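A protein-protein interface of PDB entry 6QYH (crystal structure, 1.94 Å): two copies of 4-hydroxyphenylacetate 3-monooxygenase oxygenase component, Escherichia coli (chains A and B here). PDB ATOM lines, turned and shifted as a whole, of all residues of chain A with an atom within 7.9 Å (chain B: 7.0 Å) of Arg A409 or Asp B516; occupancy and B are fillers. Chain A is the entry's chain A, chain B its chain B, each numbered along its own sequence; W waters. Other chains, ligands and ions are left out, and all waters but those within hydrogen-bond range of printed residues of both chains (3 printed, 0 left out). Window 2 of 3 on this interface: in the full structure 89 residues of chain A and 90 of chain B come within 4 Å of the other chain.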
ATOM      1  N   ALA A 247     -22.083 -20.133  23.292  1.00  0.00           N
ATOM      2  CA  ALA A 247     -23.150 -19.136  23.413  1.00  0.00           C
ATOM      3  C   ALA A 247     -22.695 -17.692  23.198  1.00  0.00           C
ATOM      4  O   ALA A 247     -23.473 -16.873  22.703  1.00  0.00           O
ATOM      5  CB  ALA A 247     -23.816 -19.266  24.784  1.00  0.00           C
ATOM      6  N   THR A 248     -21.473 -17.352  23.639  1.00  0.00           N
ATOM      7  CA  THR A 248     -20.970 -15.970  23.600  1.00  0.00           C
ATOM      8  C   THR A 248     -19.642 -15.818  22.861  1.00  0.00           C
ATOM      9  O   THR A 248     -19.077 -14.725  22.832  1.00  0.00           O
ATOM     10  CB  THR A 248     -20.888 -15.397  25.044  1.00  0.00           C
ATOM     11  OG1 THR A 248     -19.952 -16.164  25.809  1.00  0.00           O
ATOM     12  CG2 THR A 248     -22.245 -15.375  25.759  1.00  0.00           C
ATOM     13  N   GLY A 249     -19.138 -16.903  22.285  1.00  0.00           N
ATOM     14  CA  GLY A 249     -17.863 -16.870  21.576  1.00  0.00           C
ATOM     15  C   GLY A 249     -17.938 -17.654  20.285  1.00  0.00           C
ATOM     16  O   GLY A 249     -19.006 -17.779  19.699  1.00  0.00           O
ATOM     17  N   SER A 250     -16.814 -18.223  19.857  1.00  0.00           N
ATOM     18  CA  SER A 250     -16.750 -19.038  18.645  1.00  0.00           C
ATOM     19  C   SER A 250     -15.482 -19.923  18.761  1.00  0.00           C
ATOM     20  O   SER A 250     -14.635 -19.655  19.623  1.00  0.00           O
ATOM     21  CB  SER A 250     -16.648 -18.142  17.402  1.00  0.00           C
ATOM     22  OG  SER A 250     -15.377 -17.513  17.318  1.00  0.00           O
ATOM     23  N   TYR A 252     -12.918 -19.793  16.850  1.00  0.00           N
ATOM     24  CA  TYR A 252     -11.801 -18.855  16.622  1.00  0.00           C
ATOM     25  C   TYR A 252     -11.378 -18.126  17.918  1.00  0.00           C
ATOM     26  O   TYR A 252     -10.178 -17.922  18.178  1.00  0.00           O
ATOM     27  CB  TYR A 252     -12.194 -17.835  15.521  1.00  0.00           C
ATOM     28  CG  TYR A 252     -11.113 -16.829  15.175  1.00  0.00           C
ATOM     29  CD1 TYR A 252     -10.190 -17.087  14.158  1.00  0.00           C
ATOM     30  CD2 TYR A 252     -11.064 -15.584  15.805  1.00  0.00           C
ATOM     31  CE1 TYR A 252      -9.236 -16.137  13.792  1.00  0.00           C
ATOM     32  CE2 TYR A 252     -10.088 -14.642  15.472  1.00  0.00           C
ATOM     33  CZ  TYR A 252      -9.164 -14.933  14.479  1.00  0.00           C
ATOM     34  OH  TYR A 252      -8.211 -14.003  14.143  1.00  0.00           O
ATOM     35  N   ASP A 253     -12.370 -17.715  18.706  1.00  0.00           N
ATOM     36  CA  ASP A 253     -12.167 -16.970  19.946  1.00  0.00           C
ATOM     37  C   ASP A 253     -11.761 -17.856  21.123  1.00  0.00           C
ATOM     38  O   ASP A 253     -10.950 -17.438  21.934  1.00  0.00           O
ATOM     39  CB  ASP A 253     -13.431 -16.167  20.272  1.00  0.00           C
ATOM     40  CG  ASP A 253     -13.699 -15.134  19.190  1.00  0.00           C
ATOM     41  OD1 ASP A 253     -12.822 -14.267  18.973  1.00  0.00           O
ATOM     42  OD2 ASP A 253     -14.772 -15.216  18.540  1.00  0.00           O
ATOM     43  N   PRO A 405      -9.165  -8.078  19.971  1.00  0.00           N
ATOM     44  CA  PRO A 405     -10.566  -7.759  19.608  1.00  0.00           C
ATOM     45  C   PRO A 405     -11.488  -8.854  20.118  1.00  0.00           C
ATOM     46  O   PRO A 405     -11.085 -10.012  20.218  1.00  0.00           O
ATOM     47  CB  PRO A 405     -10.558  -7.689  18.077  1.00  0.00           C
ATOM     48  CG  PRO A 405      -9.260  -8.269  17.657  1.00  0.00           C
ATOM     49  CD  PRO A 405      -8.290  -8.078  18.783  1.00  0.00           C
ATOM     50  N   SER A 406     -12.688  -8.459  20.513  1.00  0.00           N
ATOM     51  CA  SER A 406     -13.687  -9.305  21.134  1.00  0.00           C
ATOM     52  C   SER A 406     -14.026 -10.603  20.443  1.00  0.00           C
ATOM     53  O   SER A 406     -14.284 -11.590  21.125  1.00  0.00           O
ATOM     54  CB  SER A 406     -14.985  -8.522  21.340  1.00  0.00           C
ATOM     55  OG  SER A 406     -15.651  -8.185  20.131  1.00  0.00           O
ATOM     56  N   SER A 407     -14.093 -10.596  19.108  1.00  0.00           N
ATOM     57  CA  SER A 407     -14.736 -11.689  18.393  1.00  0.00           C
ATOM     58  C   SER A 407     -14.293 -11.860  16.948  1.00  0.00           C
ATOM     59  O   SER A 407     -13.851 -10.907  16.317  1.00  0.00           O
ATOM     60  CB  SER A 407     -16.233 -11.335  18.381  1.00  0.00           C
ATOM     61  OG  SER A 407     -17.115 -12.302  17.838  1.00  0.00           O
ATOM     62  N   ALA A 408     -14.525 -13.067  16.391  1.00  0.00           N
ATOM     63  CA  ALA A 408     -14.399 -13.364  14.962  1.00  0.00           C
ATOM     64  C   ALA A 408     -15.412 -12.409  14.209  1.00  0.00           C
ATOM     65  O   ALA A 408     -15.162 -12.040  13.072  1.00  0.00           O
ATOM     66  CB  ALA A 408     -14.765 -14.822  14.701  1.00  0.00           C
ATOM     67  N   ARG A 409     -16.495 -11.954  14.883  1.00  0.00           N
ATOM     68  CA  ARG A 409     -17.471 -10.980  14.342  1.00  0.00           C
ATOM     69  C   ARG A 409     -16.804  -9.652  13.971  1.00  0.00           C
ATOM     70  O   ARG A 409     -17.234  -9.018  13.005  1.00  0.00           O
ATOM     71  CB  ARG A 409     -18.621 -10.719  15.321  1.00  0.00           C
ATOM     72  CG  ARG A 409     -19.506 -11.947  15.535  1.00  0.00           C
ATOM     73  CD  ARG A 409     -20.333 -11.742  16.778  1.00  0.00           C
ATOM     74  NE  ARG A 409     -21.394 -12.733  16.844  1.00  0.00           N
ATOM     75  CZ  ARG A 409     -22.628 -12.542  16.395  1.00  0.00           C
ATOM     76  NH1 ARG A 409     -22.990 -11.363  15.911  1.00  0.00           N
ATOM     77  NH2 ARG A 409     -23.525 -13.506  16.485  1.00  0.00           N
ATOM     78  N   ASP A 410     -15.754  -9.237  14.726  1.00  0.00           N
ATOM     79  CA  ASP A 410     -14.977  -8.019  14.443  1.00  0.00           C
ATOM     80  C   ASP A 410     -14.212  -8.146  13.112  1.00  0.00           C
ATOM     81  O   ASP A 410     -14.119  -7.181  12.355  1.00  0.00           O
ATOM     82  CB  ASP A 410     -13.997  -7.724  15.566  1.00  0.00           C
ATOM     83  CG  ASP A 410     -14.667  -7.423  16.893  1.00  0.00           C
ATOM     84  OD1 ASP A 410     -15.681  -6.660  16.900  1.00  0.00           O
ATOM     85  OD2 ASP A 410     -14.182  -7.935  17.925  1.00  0.00           O
ATOM     86  N   LEU A 411     -13.687  -9.340  12.827  1.00  0.00           N
ATOM     87  CA  LEU A 411     -12.961  -9.606  11.581  1.00  0.00           C
ATOM     88  C   LEU A 411     -13.918  -9.664  10.416  1.00  0.00           C
ATOM     89  O   LEU A 411     -13.529  -9.340   9.300  1.00  0.00           O
ATOM     90  CB  LEU A 411     -12.211 -10.948  11.650  1.00  0.00           C
ATOM     91  CG  LEU A 411     -11.142 -11.135  12.685  1.00  0.00           C
ATOM     92  CD1 LEU A 411     -10.671 -12.549  12.625  1.00  0.00           C
ATOM     93  CD2 LEU A 411      -9.959 -10.184  12.447  1.00  0.00           C
ATOM     94  N   ASN A 412     -15.166 -10.084  10.674  1.00  0.00           N
ATOM     95  CA  ASN A 412     -16.196 -10.216   9.659  1.00  0.00           C
ATOM     96  C   ASN A 412     -16.962  -8.896   9.410  1.00  0.00           C
ATOM     97  O   ASN A 412     -17.810  -8.843   8.539  1.00  0.00           O
ATOM     98  CB  ASN A 412     -17.115 -11.414   9.984  1.00  0.00           C
ATOM     99  CG  ASN A 412     -16.360 -12.745   9.895  1.00  0.00           C
ATOM    100  OD1 ASN A 412     -15.424 -12.908   9.103  1.00  0.00           O
ATOM    101  ND2 ASN A 412     -16.719 -13.721  10.717  1.00  0.00           N
ATOM    102  N   ASN A 413     -16.627  -7.821  10.138  1.00  0.00           N
ATOM    103  CA  ASN A 413     -17.217  -6.499   9.920  1.00  0.00           C
ATOM    104  C   ASN A 413     -16.109  -5.666   9.262  1.00  0.00           C
ATOM    105  O   ASN A 413     -15.123  -5.341   9.927  1.00  0.00           O
ATOM    106  CB  ASN A 413     -17.717  -5.852  11.234  1.00  0.00           C
ATOM    107  CG  ASN A 413     -18.272  -4.443  11.067  1.00  0.00           C
ATOM    108  OD1 ASN A 413     -18.012  -3.741  10.080  1.00  0.00           O
ATOM    109  ND2 ASN A 413     -19.050  -3.987  12.035  1.00  0.00           N
ATOM    110  N   PRO A 414     -16.254  -5.302   7.956  1.00  0.00           N
ATOM    111  CA  PRO A 414     -15.177  -4.550   7.273  1.00  0.00           C
ATOM    112  C   PRO A 414     -14.804  -3.201   7.909  1.00  0.00           C
ATOM    113  O   PRO A 414     -13.649  -2.804   7.794  1.00  0.00           O
ATOM    114  CB  PRO A 414     -15.688  -4.404   5.833  1.00  0.00           C
ATOM    115  CG  PRO A 414     -16.780  -5.407   5.691  1.00  0.00           C
ATOM    116  CD  PRO A 414     -17.376  -5.604   7.036  1.00  0.00           C
ATOM    117  N   ILE A 416     -14.570  -2.529  11.110  1.00  0.00           N
ATOM    118  CA  ILE A 416     -13.633  -2.828  12.199  1.00  0.00           C
ATOM    119  C   ILE A 416     -12.376  -3.477  11.611  1.00  0.00           C
ATOM    120  O   ILE A 416     -11.255  -3.117  11.978  1.00  0.00           O
ATOM    121  CB  ILE A 416     -14.290  -3.761  13.264  1.00  0.00           C
ATOM    122  CG1 ILE A 416     -15.563  -3.122  13.851  1.00  0.00           C
ATOM    123  CG2 ILE A 416     -13.278  -4.160  14.363  1.00  0.00           C
ATOM    124  CD1 ILE A 416     -16.544  -4.107  14.480  1.00  0.00           C
ATOM    125  N   ASP A 417     -12.575  -4.465  10.729  1.00  0.00           N
ATOM    126  CA  ASP A 417     -11.503  -5.246  10.130  1.00  0.00           C
ATOM    127  C   ASP A 417     -10.413  -4.408   9.449  1.00  0.00           C
ATOM    128  O   ASP A 417      -9.241  -4.771   9.513  1.00  0.00           O
ATOM    129  CB  ASP A 417     -12.063  -6.280   9.151  1.00  0.00           C
ATOM    130  CG  ASP A 417     -11.011  -7.327   8.810  1.00  0.00           C
ATOM    131  OD1 ASP A 417     -10.499  -7.972   9.738  1.00  0.00           O
ATOM    132  OD2 ASP A 417     -10.679  -7.466   7.619  1.00  0.00           O
ATOM    133  N   LEU A 420      -7.980  -3.381  12.126  1.00  0.00           N
ATOM    134  CA  LEU A 420      -7.229  -4.542  12.611  1.00  0.00           C
ATOM    135  C   LEU A 420      -6.143  -4.931  11.600  1.00  0.00           C
ATOM    136  O   LEU A 420      -5.016  -5.212  12.002  1.00  0.00           O
ATOM    137  CB  LEU A 420      -8.168  -5.728  12.925  1.00  0.00           C
ATOM    138  CG  LEU A 420      -9.240  -5.487  14.012  1.00  0.00           C
ATOM    139  CD1 LEU A 420     -10.164  -6.690  14.162  1.00  0.00           C
ATOM    140  CD2 LEU A 420      -8.612  -5.103  15.374  1.00  0.00           C
ATOM    141  N   GLN B 498     -12.137 -18.211  11.155  1.00  0.00           N
ATOM    142  CA  GLN B 498     -13.068 -17.160  11.590  1.00  0.00           C
ATOM    143  C   GLN B 498     -14.545 -17.492  11.315  1.00  0.00           C
ATOM    144  O   GLN B 498     -15.425 -16.827  11.861  1.00  0.00           O
ATOM    145  CB  GLN B 498     -12.674 -15.789  11.005  1.00  0.00           C
ATOM    146  CG  GLN B 498     -12.963 -15.619   9.511  1.00  0.00           C
ATOM    147  CD  GLN B 498     -12.111 -14.520   8.923  1.00  0.00           C
ATOM    148  OE1 GLN B 498     -10.933 -14.716   8.605  1.00  0.00           O
ATOM    149  NE2 GLN B 498     -12.683 -13.341   8.760  1.00  0.00           N
ATOM    150  N   ASN B 513     -25.299 -19.804  19.645  1.00  0.00           N
ATOM    151  CA  ASN B 513     -24.735 -18.462  19.812  1.00  0.00           C
ATOM    152  C   ASN B 513     -25.867 -17.445  19.926  1.00  0.00           C
ATOM    153  O   ASN B 513     -26.711 -17.374  19.054  1.00  0.00           O
ATOM    154  CB  ASN B 513     -23.716 -18.103  18.731  1.00  0.00           C
ATOM    155  CG  ASN B 513     -22.990 -16.812  19.058  1.00  0.00           C
ATOM    156  OD1 ASN B 513     -23.511 -15.719  18.848  1.00  0.00           O
ATOM    157  ND2 ASN B 513     -21.791 -16.916  19.594  1.00  0.00           N
ATOM    158  N   MET B 514     -25.884 -16.684  21.038  1.00  0.00           N
ATOM    159  CA  MET B 514     -26.925 -15.709  21.377  1.00  0.00           C
ATOM    160  C   MET B 514     -26.585 -14.238  21.106  1.00  0.00           C
ATOM    161  O   MET B 514     -27.406 -13.377  21.434  1.00  0.00           O
ATOM    162  CB  MET B 514     -27.335 -15.873  22.859  1.00  0.00           C
ATOM    163  CG  MET B 514     -26.242 -15.505  23.853  1.00  0.00           C
ATOM    164  SD  MET B 514     -26.424 -16.340  25.466  1.00  0.00           S
ATOM    165  CE  MET B 514     -27.774 -15.380  26.167  1.00  0.00           C
ATOM    166  N   LEU B 515     -25.404 -13.946  20.529  1.00  0.00           N
ATOM    167  CA  LEU B 515     -24.945 -12.564  20.273  1.00  0.00           C
ATOM    168  C   LEU B 515     -25.833 -11.750  19.308  1.00  0.00           C
ATOM    169  O   LEU B 515     -26.092 -10.593  19.628  1.00  0.00           O
ATOM    170  CB  LEU B 515     -23.474 -12.502  19.855  1.00  0.00           C
ATOM    171  CG  LEU B 515     -22.473 -13.151  20.835  1.00  0.00           C
ATOM    172  CD1 LEU B 515     -21.064 -13.058  20.323  1.00  0.00           C
ATOM    173  CD2 LEU B 515     -22.568 -12.561  22.203  1.00  0.00           C
ATOM    174  N   ASP B 516     -26.363 -12.345  18.214  1.00  0.00           N
ATOM    175  CA  ASP B 516     -27.281 -11.622  17.306  1.00  0.00           C
ATOM    176  C   ASP B 516     -28.545 -11.173  18.039  1.00  0.00           C
ATOM    177  O   ASP B 516     -28.964 -10.020  17.896  1.00  0.00           O
ATOM    178  CB  ASP B 516     -27.695 -12.487  16.102  1.00  0.00           C
ATOM    179  CG  ASP B 516     -26.588 -12.764  15.101  1.00  0.00           C
ATOM    180  OD1 ASP B 516     -25.694 -11.906  14.947  1.00  0.00           O
ATOM    181  OD2 ASP B 516     -26.626 -13.830  14.460  1.00  0.00           O
ATOM    182  N   LYS B 517     -29.139 -12.086  18.835  1.00  0.00           N
ATOM    183  CA  LYS B 517     -30.356 -11.830  19.617  1.00  0.00           C
ATOM    184  C   LYS B 517     -30.119 -10.800  20.719  1.00  0.00           C
ATOM    185  O   LYS B 517     -30.988  -9.975  20.979  1.00  0.00           O
ATOM    186  CB  LYS B 517     -30.920 -13.141  20.197  1.00  0.00           C
ATOM    187  CG  LYS B 517     -31.565 -14.047  19.145  1.00  0.00           C
ATOM    188  CD  LYS B 517     -31.967 -15.409  19.700  1.00  0.00           C
ATOM    189  CE  LYS B 517     -32.554 -16.279  18.615  1.00  0.00           C
ATOM    190  NZ  LYS B 517     -33.137 -17.530  19.163  1.00  0.00           N
ATOM    191  N   LEU B 518     -28.927 -10.814  21.321  1.00  0.00           N
ATOM    192  CA  LEU B 518     -28.531  -9.921  22.407  1.00  0.00           C
ATOM    193  C   LEU B 518     -28.164  -8.507  21.968  1.00  0.00           C
ATOM    194  O   LEU B 518     -28.426  -7.559  22.710  1.00  0.00           O
ATOM    195  CB  LEU B 518     -27.332 -10.535  23.152  1.00  0.00           C
ATOM    196  CG  LEU B 518     -27.268 -10.322  24.649  1.00  0.00           C
ATOM    197  CD1 LEU B 518     -28.406 -11.035  25.339  1.00  0.00           C
ATOM    198  CD2 LEU B 518     -25.968 -10.843  25.198  1.00  0.00           C
ATOM    199  N   LEU B 519     -27.459  -8.373  20.834  1.00  0.00           N
ATOM    200  CA  LEU B 519     -26.960  -7.077  20.351  1.00  0.00           C
ATOM    201  C   LEU B 519     -27.876  -6.499  19.285  1.00  0.00           C
ATOM    202  O   LEU B 519     -28.804  -7.198  18.897  1.00  0.00           O
ATOM    203  CB  LEU B 519     -25.528  -7.229  19.830  1.00  0.00           C
ATOM    204  CG  LEU B 519     -24.536  -7.908  20.787  1.00  0.00           C
ATOM    205  CD1 LEU B 519     -23.395  -8.482  20.038  1.00  0.00           C
ATOM    206  CD2 LEU B 519     -24.053  -6.980  21.875  1.00  0.00           C
ATOM    207  N   LYS B 520     -27.616  -5.270  18.785  1.00  0.00           N
ATOM    208  CA  LYS B 520     -28.436  -4.590  17.746  1.00  0.00           C
ATOM    209  C   LYS B 520     -29.824  -4.200  18.283  1.00  0.00           C
ATOM    210  O   LYS B 520     -29.945  -3.574  19.338  1.00  0.00           O
ATOM    211  CB  LYS B 520     -28.595  -5.421  16.435  1.00  0.00           C
ATOM    212  CG  LYS B 520     -27.298  -5.896  15.765  1.00  0.00           C
ATOM    213  CD  LYS B 520     -27.029  -7.395  15.988  1.00  0.00           C
ATOM    214  CE  LYS B 520     -27.549  -8.292  14.886  1.00  0.00           C
ATOM    215  NZ  LYS B 520     -26.571  -8.441  13.773  1.00  0.00           N
HETATM  216  O   HOH W   1     -19.492 -15.059  18.198  1.00  0.00           O
HETATM  217  O   HOH W   2     -10.955 -10.698   7.848  1.00  0.00           O
HETATM  218  O   HOH W   3     -25.749 -15.002  17.188  1.00  0.00           O
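No position is printed for both chains.
Water W3 lies within hydrogen-bond range of NH2 of Arg A409, OD1 of Asn B513 and N of Asp B516.
Water W1 lies within hydrogen-bond range of the backbone carbonyl oxygen (O) of Gly A249 (3.1 Å), the side-chain amide nitrogen (ND2) of Asn B513 (3.3 Å) and the guanidinium group (NE) of Arg A409 (3.3 Å).
Water W2 lies within hydrogen-bond range of the side-chain carboxylate (OD2) of Asp A417 (3.3 Å), the backbone carbonyl oxygen (O) of Leu A411 (3.3 Å) and the side-chain amide nitrogen (NE2) of Gln B498 (3.3 Å).
OG of Ser A250 lies close to N of Tyr A252 (3.4 Å).
N of Ala A408 is in hydrogen-bond range of OD2 of Asp A253, at 3.0 Å.
The side-chain hydroxyl of Ser A407 sits close to the backbone NH of Arg A409.
ND2 of Asn A412 is in hydrogen-bond range of O of Ala A408 (3.3 Å).
The side-chain amide oxygen of Asn B513 lies within hydrogen-bond range of the backbone NH of Leu B515 (3.1 Å).
OD1 of Asp B516 is in salt-bridge range of NZ of Lys B520, at 3.8 Å.
Hydrophobic or aromatic side chains of chain A within 4 Å of the printed part of chain B: Ala A247, Tyr A252, Ala A408 and Leu A411.
Hydrophobic or aromatic side chains of chain B within 4 Å of the printed part of chain A: Met B514 and Leu B515.
Among the printed residues, Asp or Glu carboxylates within 4 Å of a Lys or Arg side-chain nitrogen of the other chain: Arg A409 with Asp B516 (2.9 Å).
Among the printed residues, merely in contact across the chains: Arg A409 with Leu B515 (3.5 Å), Ala A247 with Asn B513 (3.5 Å), Ala A408 with Gln B498 (3.5 Å), Thr A248 with Leu B515 (3.6 Å), Tyr A252 with Gln B498 (3.8 Å) and Leu A411 with Gln B498 (3.8 Å).
The backbone carbonyl oxygen (O) of Ala A247 lies within hydrogen-bond range of the backbone NH (N) of Met B514 (2.9 Å).
O of Gly A249 is in hydrogen-bond range of ND2 of Asn B513 (2.9 Å).
NH2 of Arg A409 lies within hydrogen-bond range of OD1 of Asn B513, at 3.2 Å.
NH1 of Arg A409 lies within salt-bridge range of OD1 of Asp B516, at 2.9 Å.
OD1 of Asn A412 lies within hydrogen-bond range of NE2 of Gln B498.
Of chain B, only Asn B513 (3.2 Å), Leu B515 (3.5 Å) and Asp B516 (2.9 Å) come within 4 Å of Arg A409.
Asp B516 touches just one residue of chain A: Arg A409.
Printed residues of chain B within 4 Å of Leu A411: Gln B498 (3.8 Å).
Of the printed residues of chain A, Met B514 touches Ala A247.
Of the printed residues of chain B, Asn A412 touches Gln B498.
Of the printed residues of chain A, Gln B498 touches Tyr A252, Ala A408, Leu A411 and Asn A412.
Printed residues of chain B within 4 Å of Gly A249: Asn B513.
Asp A253 touches none of the printed residues of chain B.
The nearest residue of chain B that does not touch Arg A409 is Leu B519 (5.0 Å).
The nearest printed residue of chain B that does not touch Tyr A252 is Asn B513 (9.7 Å).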
